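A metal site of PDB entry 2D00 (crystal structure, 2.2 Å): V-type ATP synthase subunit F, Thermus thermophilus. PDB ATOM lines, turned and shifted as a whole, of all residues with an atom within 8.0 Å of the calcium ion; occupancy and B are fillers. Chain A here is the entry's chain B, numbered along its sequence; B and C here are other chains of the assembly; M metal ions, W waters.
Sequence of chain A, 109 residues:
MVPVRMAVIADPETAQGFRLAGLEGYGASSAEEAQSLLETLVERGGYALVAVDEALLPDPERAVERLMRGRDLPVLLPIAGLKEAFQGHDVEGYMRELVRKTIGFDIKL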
ATOM      1  N   GLU A  39       5.506   8.440 -13.451  1.00  0.00           N
ATOM      2  CA  GLU A  39       6.682   7.766 -12.910  1.00  0.00           C
ATOM      3  C   GLU A  39       6.746   6.352 -13.563  1.00  0.00           C
ATOM      4  O   GLU A  39       7.458   6.175 -14.540  1.00  0.00           O
ATOM      5  CB  GLU A  39       6.627   7.815 -11.354  1.00  0.00           C
ATOM      6  CG  GLU A  39       7.709   6.947 -10.529  1.00  0.00           C
ATOM      7  CD  GLU A  39       9.170   7.360 -10.752  1.00  0.00           C
ATOM      8  OE1 GLU A  39       9.424   8.585 -10.900  1.00  0.00           O
ATOM      9  OE2 GLU A  39      10.069   6.446 -10.768  1.00  0.00           O
ATOM     10  N   GLU A  43      10.258   5.358 -16.868  1.00  0.00           N
ATOM     11  CA  GLU A  43      11.274   4.409 -16.693  1.00  0.00           C
ATOM     12  C   GLU A  43      11.134   3.254 -17.742  1.00  0.00           C
ATOM     13  O   GLU A  43      12.005   2.365 -17.817  1.00  0.00           O
ATOM     14  CB  GLU A  43      11.186   3.904 -15.232  1.00  0.00           C
ATOM     15  CG  GLU A  43       9.879   3.232 -14.864  1.00  0.00           C
ATOM     16  CD  GLU A  43       9.773   2.849 -13.436  1.00  0.00           C
ATOM     17  OE1 GLU A  43       9.953   3.734 -12.560  1.00  0.00           O
ATOM     18  OE2 GLU A  43       9.474   1.637 -13.199  1.00  0.00           O
ATOM     19  N   ARG A  66      10.332  16.564 -10.579  1.00  0.00           N
ATOM     20  CA  ARG A  66       9.961  15.403  -9.723  1.00  0.00           C
ATOM     21  C   ARG A  66      10.449  14.025 -10.256  1.00  0.00           C
ATOM     22  O   ARG A  66      11.009  13.172  -9.505  1.00  0.00           O
ATOM     23  CB  ARG A  66       8.401  15.410  -9.507  1.00  0.00           C
ATOM     24  CG  ARG A  66       8.030  16.337  -8.308  1.00  0.00           C
ATOM     25  CD  ARG A  66       6.597  16.672  -8.189  1.00  0.00           C
ATOM     26  NE  ARG A  66       5.800  15.474  -8.074  1.00  0.00           N
ATOM     27  CZ  ARG A  66       4.489  15.464  -7.832  1.00  0.00           C
ATOM     28  NH1 ARG A  66       3.878  16.643  -7.661  1.00  0.00           N
ATOM     29  NH2 ARG A  66       3.786  14.306  -7.782  1.00  0.00           N
ATOM     30  N   LEU A  67      10.240  13.829 -11.569  1.00  0.00           N
ATOM     31  CA  LEU A  67      10.669  12.593 -12.238  1.00  0.00           C
ATOM     32  C   LEU A  67      12.157  12.417 -12.397  1.00  0.00           C
ATOM     33  O   LEU A  67      12.642  11.309 -12.355  1.00  0.00           O
ATOM     34  CB  LEU A  67      10.037  12.468 -13.611  1.00  0.00           C
ATOM     35  CG  LEU A  67       8.571  12.004 -13.517  1.00  0.00           C
ATOM     36  CD1 LEU A  67       7.866  12.380 -14.838  1.00  0.00           C
ATOM     37  CD2 LEU A  67       8.499  10.538 -13.180  1.00  0.00           C
ATOM     38  N   MET A  68      12.886  13.518 -12.593  1.00  0.00           N
ATOM     39  CA  MET A  68      14.268  13.442 -12.609  1.00  0.00           C
ATOM     40  C   MET A  68      14.709  12.932 -11.206  1.00  0.00           C
ATOM     41  O   MET A  68      15.389  11.898 -11.095  1.00  0.00           O
ATOM     42  CB  MET A  68      14.818  14.829 -12.951  1.00  0.00           C
ATOM     43  CG  MET A  68      14.651  15.104 -14.448  1.00  0.00           C
ATOM     44  SD  MET A  68      15.530  16.524 -15.164  1.00  0.00           S
ATOM     45  CE  MET A  68      14.766  16.579 -16.789  1.00  0.00           C
ATOM     46  N   ARG A  69      14.275  13.631 -10.148  1.00  0.00           N
ATOM     47  CA  ARG A  69      14.690  13.325  -8.774  1.00  0.00           C
ATOM     48  C   ARG A  69      14.277  11.927  -8.228  1.00  0.00           C
ATOM     49  O   ARG A  69      14.493  11.563  -7.093  1.00  0.00           O
ATOM     50  CB  ARG A  69      14.174  14.443  -7.851  1.00  0.00           C
ATOM     51  CG  ARG A  69      14.845  15.810  -8.105  1.00  0.00           C
ATOM     52  CD  ARG A  69      14.328  16.931  -7.168  1.00  0.00           C
ATOM     53  NE  ARG A  69      15.296  18.030  -6.979  1.00  0.00           N
ATOM     54  CZ  ARG A  69      16.295  18.032  -6.090  1.00  0.00           C
ATOM     55  NH1 ARG A  69      16.492  17.007  -5.237  1.00  0.00           N
ATOM     56  NH2 ARG A  69      17.116  19.086  -6.029  1.00  0.00           N
ATOM     57  N   GLY A  70      13.697  11.112  -9.068  1.00  0.00           N
ATOM     58  CA  GLY A  70      13.075   9.826  -8.659  1.00  0.00           C
ATOM     59  C   GLY A  70      14.012   8.650  -8.952  1.00  0.00           C
ATOM     60  O   GLY A  70      13.801   7.563  -8.429  1.00  0.00           O
ATOM     61  N   ARG A  71      15.032   8.863  -9.776  1.00  0.00           N
ATOM     62  CA  ARG A  71      15.951   7.866 -10.114  1.00  0.00           C
ATOM     63  C   ARG A  71      16.744   7.355  -8.859  1.00  0.00           C
ATOM     64  O   ARG A  71      17.382   8.171  -8.130  1.00  0.00           O
ATOM     65  CB  ARG A  71      16.905   8.456 -11.171  1.00  0.00           C
ATOM     66  CG  ARG A  71      17.329   7.364 -12.253  1.00  0.00           C
ATOM     67  CD  ARG A  71      18.434   7.947 -13.209  1.00  0.00           C
ATOM     68  NE  ARG A  71      18.663   7.034 -14.344  1.00  0.00           N
ATOM     69  CZ  ARG A  71      19.661   7.148 -15.201  1.00  0.00           C
ATOM     70  NH1 ARG A  71      20.560   8.165 -15.111  1.00  0.00           N
ATOM     71  NH2 ARG A  71      19.805   6.228 -16.155  1.00  0.00           N
ATOM     72  N   ASP A  72      16.698   6.047  -8.609  1.00  0.00           N
ATOM     73  CA  ASP A  72      17.573   5.345  -7.635  1.00  0.00           C
ATOM     74  C   ASP A  72      19.029   5.338  -8.099  1.00  0.00           C
ATOM     75  O   ASP A  72      19.314   4.975  -9.224  1.00  0.00           O
ATOM     76  CB  ASP A  72      17.058   3.954  -7.252  1.00  0.00           C
ATOM     77  CG  ASP A  72      15.791   4.047  -6.375  1.00  0.00           C
ATOM     78  OD1 ASP A  72      15.249   5.163  -6.373  1.00  0.00           O
ATOM     79  OD2 ASP A  72      15.334   3.099  -5.670  1.00  0.00           O
ATOM     80  N   LEU A  73      19.915   5.860  -7.274  1.00  0.00           N
ATOM     81  CA  LEU A  73      21.289   6.006  -7.559  1.00  0.00           C
ATOM     82  C   LEU A  73      22.171   5.080  -6.662  1.00  0.00           C
ATOM     83  O   LEU A  73      21.916   4.922  -5.517  1.00  0.00           O
ATOM     84  CB  LEU A  73      21.651   7.402  -7.327  1.00  0.00           C
ATOM     85  CG  LEU A  73      21.156   8.413  -8.328  1.00  0.00           C
ATOM     86  CD1 LEU A  73      22.050   9.601  -8.207  1.00  0.00           C
ATOM     87  CD2 LEU A  73      21.274   7.958  -9.674  1.00  0.00           C
ATOM     88  N   ILE B   9      10.855   0.002   1.086  1.00  0.00           N
ATOM     89  CA  ILE B   9      10.682   1.343   0.527  1.00  0.00           C
ATOM     90  C   ILE B   9      10.982   2.404   1.660  1.00  0.00           C
ATOM     91  O   ILE B   9      10.348   2.429   2.711  1.00  0.00           O
ATOM     92  CB  ILE B   9       9.284   1.600  -0.053  1.00  0.00           C
ATOM     93  CG1 ILE B   9       9.010   0.615  -1.177  1.00  0.00           C
ATOM     94  CG2 ILE B   9       9.156   2.976  -0.666  1.00  0.00           C
ATOM     95  CD1 ILE B   9       7.650   0.744  -1.735  1.00  0.00           C
ATOM     96  N   ALA B  10      12.055   3.181   1.416  1.00  0.00           N
ATOM     97  CA  ALA B  10      12.484   4.204   2.374  1.00  0.00           C
ATOM     98  C   ALA B  10      12.933   5.430   1.700  1.00  0.00           C
ATOM     99  O   ALA B  10      13.013   5.461   0.477  1.00  0.00           O
ATOM    100  CB  ALA B  10      13.593   3.639   3.271  1.00  0.00           C
ATOM    101  N   ASP B  11      13.292   6.451   2.463  1.00  0.00           N
ATOM    102  CA  ASP B  11      13.935   7.637   1.880  1.00  0.00           C
ATOM    103  C   ASP B  11      15.209   7.272   1.036  1.00  0.00           C
ATOM    104  O   ASP B  11      15.873   6.226   1.293  1.00  0.00           O
ATOM    105  CB  ASP B  11      14.292   8.650   3.000  1.00  0.00           C
ATOM    106  CG  ASP B  11      15.479   8.204   3.851  1.00  0.00           C
ATOM    107  OD1 ASP B  11      15.252   7.716   4.992  1.00  0.00           O
ATOM    108  OD2 ASP B  11      16.675   8.366   3.408  1.00  0.00           O
ATOM    109  N   PRO B  12      15.555   8.059   0.028  1.00  0.00           N
ATOM    110  CA  PRO B  12      16.630   7.594  -0.859  1.00  0.00           C
ATOM    111  C   PRO B  12      17.983   7.185  -0.216  1.00  0.00           C
ATOM    112  O   PRO B  12      18.556   6.200  -0.654  1.00  0.00           O
ATOM    113  CB  PRO B  12      16.827   8.791  -1.782  1.00  0.00           C
ATOM    114  CG  PRO B  12      15.397   9.403  -1.842  1.00  0.00           C
ATOM    115  CD  PRO B  12      15.051   9.373  -0.405  1.00  0.00           C
ATOM    116  N   ALA B  15      17.328   3.926   1.569  1.00  0.00           N
ATOM    117  CA  ALA B  15      17.209   2.889   0.585  1.00  0.00           C
ATOM    118  C   ALA B  15      18.616   2.429   0.113  1.00  0.00           C
ATOM    119  O   ALA B  15      18.862   1.258   0.029  1.00  0.00           O
ATOM    120  CB  ALA B  15      16.439   3.414  -0.555  1.00  0.00           C
ATOM    121  N   TYR B  26      14.326   0.470  -2.023  1.00  0.00           N
ATOM    122  CA  TYR B  26      13.993   1.369  -3.117  1.00  0.00           C
ATOM    123  C   TYR B  26      13.706   2.764  -2.424  1.00  0.00           C
ATOM    124  O   TYR B  26      13.093   2.842  -1.359  1.00  0.00           O
ATOM    125  CB  TYR B  26      12.680   0.842  -3.771  1.00  0.00           C
ATOM    126  CG  TYR B  26      12.863  -0.401  -4.527  1.00  0.00           C
ATOM    127  CD1 TYR B  26      13.306  -0.359  -5.826  1.00  0.00           C
ATOM    128  CD2 TYR B  26      12.553  -1.656  -3.957  1.00  0.00           C
ATOM    129  CE1 TYR B  26      13.521  -1.486  -6.558  1.00  0.00           C
ATOM    130  CE2 TYR B  26      12.692  -2.803  -4.685  1.00  0.00           C
ATOM    131  CZ  TYR B  26      13.230  -2.732  -5.982  1.00  0.00           C
ATOM    132  OH  TYR B  26      13.427  -3.816  -6.782  1.00  0.00           O
ATOM    133  N   GLY B  27      14.173   3.847  -3.002  1.00  0.00           N
ATOM    134  CA  GLY B  27      14.099   5.110  -2.327  1.00  0.00           C
ATOM    135  C   GLY B  27      12.894   5.827  -2.894  1.00  0.00           C
ATOM    136  O   GLY B  27      12.588   5.806  -4.106  1.00  0.00           O
ATOM    137  N   ALA B  28      12.244   6.578  -2.055  1.00  0.00           N
ATOM    138  CA  ALA B  28      11.173   7.363  -2.550  1.00  0.00           C
ATOM    139  C   ALA B  28      11.179   8.599  -1.711  1.00  0.00           C
ATOM    140  O   ALA B  28      11.448   8.541  -0.516  1.00  0.00           O
ATOM    141  CB  ALA B  28       9.868   6.611  -2.362  1.00  0.00           C
ATOM    142  N   SER B  29      10.863   9.744  -2.382  1.00  0.00           N
ATOM    143  CA  SER B  29      10.876  11.044  -1.721  1.00  0.00           C
ATOM    144  C   SER B  29       9.445  11.550  -1.361  1.00  0.00           C
ATOM    145  O   SER B  29       9.268  12.631  -0.812  1.00  0.00           O
ATOM    146  CB  SER B  29      11.590  12.013  -2.674  1.00  0.00           C
ATOM    147  OG  SER B  29      13.001  11.522  -2.958  1.00  0.00           O
ATOM    148  N   SER B  30       8.437  10.750  -1.686  1.00  0.00           N
ATOM    149  CA  SER B  30       7.068  11.012  -1.272  1.00  0.00           C
ATOM    150  C   SER B  30       6.098   9.848  -1.404  1.00  0.00           C
ATOM    151  O   SER B  30       6.321   8.833  -2.115  1.00  0.00           O
ATOM    152  CB  SER B  30       6.525  12.215  -2.070  1.00  0.00           C
ATOM    153  OG  SER B  30       6.180  11.751  -3.385  1.00  0.00           O
ATOM    154  N   GLU B  33       5.384   8.717  -4.843  1.00  0.00           N
ATOM    155  CA  GLU B  33       6.494   7.935  -5.395  1.00  0.00           C
ATOM    156  C   GLU B  33       6.456   6.572  -4.851  1.00  0.00           C
ATOM    157  O   GLU B  33       6.617   5.608  -5.592  1.00  0.00           O
ATOM    158  CB  GLU B  33       7.907   8.474  -5.024  1.00  0.00           C
ATOM    159  CG  GLU B  33       8.230   9.707  -5.682  1.00  0.00           C
ATOM    160  CD  GLU B  33       9.742  10.074  -5.506  1.00  0.00           C
ATOM    161  OE1 GLU B  33      10.725   9.222  -5.165  1.00  0.00           O
ATOM    162  OE2 GLU B  33       9.919  11.317  -5.717  1.00  0.00           O
ATOM    163  N   ALA B  34       6.322   6.474  -3.547  1.00  0.00           N
ATOM    164  CA  ALA B  34       6.040   5.147  -2.939  1.00  0.00           C
ATOM    165  C   ALA B  34       4.943   4.356  -3.563  1.00  0.00           C
ATOM    166  O   ALA B  34       5.101   3.134  -3.782  1.00  0.00           O
ATOM    167  CB  ALA B  34       5.866   5.229  -1.465  1.00  0.00           C
ATOM    168  N   LEU B  37       6.059   2.906  -6.913  1.00  0.00           N
ATOM    169  CA  LEU B  37       6.975   1.782  -6.611  1.00  0.00           C
ATOM    170  C   LEU B  37       6.224   0.527  -6.256  1.00  0.00           C
ATOM    171  O   LEU B  37       6.513  -0.631  -6.787  1.00  0.00           O
ATOM    172  CB  LEU B  37       7.915   2.143  -5.452  1.00  0.00           C
ATOM    173  CG  LEU B  37       9.080   2.937  -5.864  1.00  0.00           C
ATOM    174  CD1 LEU B  37       9.911   3.310  -4.587  1.00  0.00           C
ATOM    175  CD2 LEU B  37       9.867   2.165  -7.056  1.00  0.00           C
ATOM    176  N   MET C  68      20.670  12.184 -12.190  1.00  0.00           N
ATOM    177  CA  MET C  68      19.240  12.572 -11.966  1.00  0.00           C
ATOM    178  C   MET C  68      18.524  13.214 -13.117  1.00  0.00           C
ATOM    179  O   MET C  68      17.253  13.098 -13.204  1.00  0.00           O
ATOM    180  CB  MET C  68      19.053  13.547 -10.788  1.00  0.00           C
ATOM    181  CG  MET C  68      19.497  13.030  -9.412  1.00  0.00           C
ATOM    182  SD  MET C  68      18.715  11.515  -8.726  1.00  0.00           S
ATOM    183  CE  MET C  68      19.216  10.358  -9.911  1.00  0.00           C
ATOM    184  N   ARG C  71      17.717  10.587 -17.083  1.00  0.00           N
ATOM    185  CA  ARG C  71      16.636   9.729 -17.446  1.00  0.00           C
ATOM    186  C   ARG C  71      16.140   9.933 -18.945  1.00  0.00           C
ATOM    187  O   ARG C  71      15.463   9.046 -19.483  1.00  0.00           O
ATOM    188  CB  ARG C  71      15.533   9.956 -16.400  1.00  0.00           C
ATOM    189  CG  ARG C  71      15.647   9.164 -15.152  1.00  0.00           C
ATOM    190  CD  ARG C  71      14.375   9.317 -14.330  1.00  0.00           C
ATOM    191  NE  ARG C  71      13.811   8.023 -13.965  1.00  0.00           N
ATOM    192  CZ  ARG C  71      12.922   7.799 -12.982  1.00  0.00           C
ATOM    193  NH1 ARG C  71      12.457   8.774 -12.206  1.00  0.00           N
ATOM    194  NH2 ARG C  71      12.507   6.567 -12.745  1.00  0.00           N
HETATM  195 CA    CA M   1      13.154   6.422  -6.363  1.00  0.00          CA
HETATM  196  O   HOH W   1      14.135   8.241  -5.362  1.00  0.00           O
HETATM  197  O   HOH W   2      12.393   5.016  -7.985  1.00  0.00           O
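The backbone NH (N) of Ser 29 of chain B sits at hydrogen-bond distance from the side-chain carboxylate (OE1) of Glu 33 of chain B. The backbone NH (N) of Glu 33 of chain B lies within hydrogen-bond range of the side-chain hydroxyl (OG) of Ser 30 of chain B, 3.5 Å away.
Residues that only touch the calcium ion: Glu 33 of chain B (3.9 Å). Of the 25 residues printed, 4 come within 4 Å of the calcium ion.
The calcium ion is bound by water W2. Water W1 is bound to the calcium ion, at 2.3 Å. The calcium ion is bound by O of Gly 27 of chain B. The calcium ion is bound by the side-chain carboxylate (OD1) of Asp 72 (2.4 Å). The calcium ion is bound by O of Gly 70 (2.4 Å).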
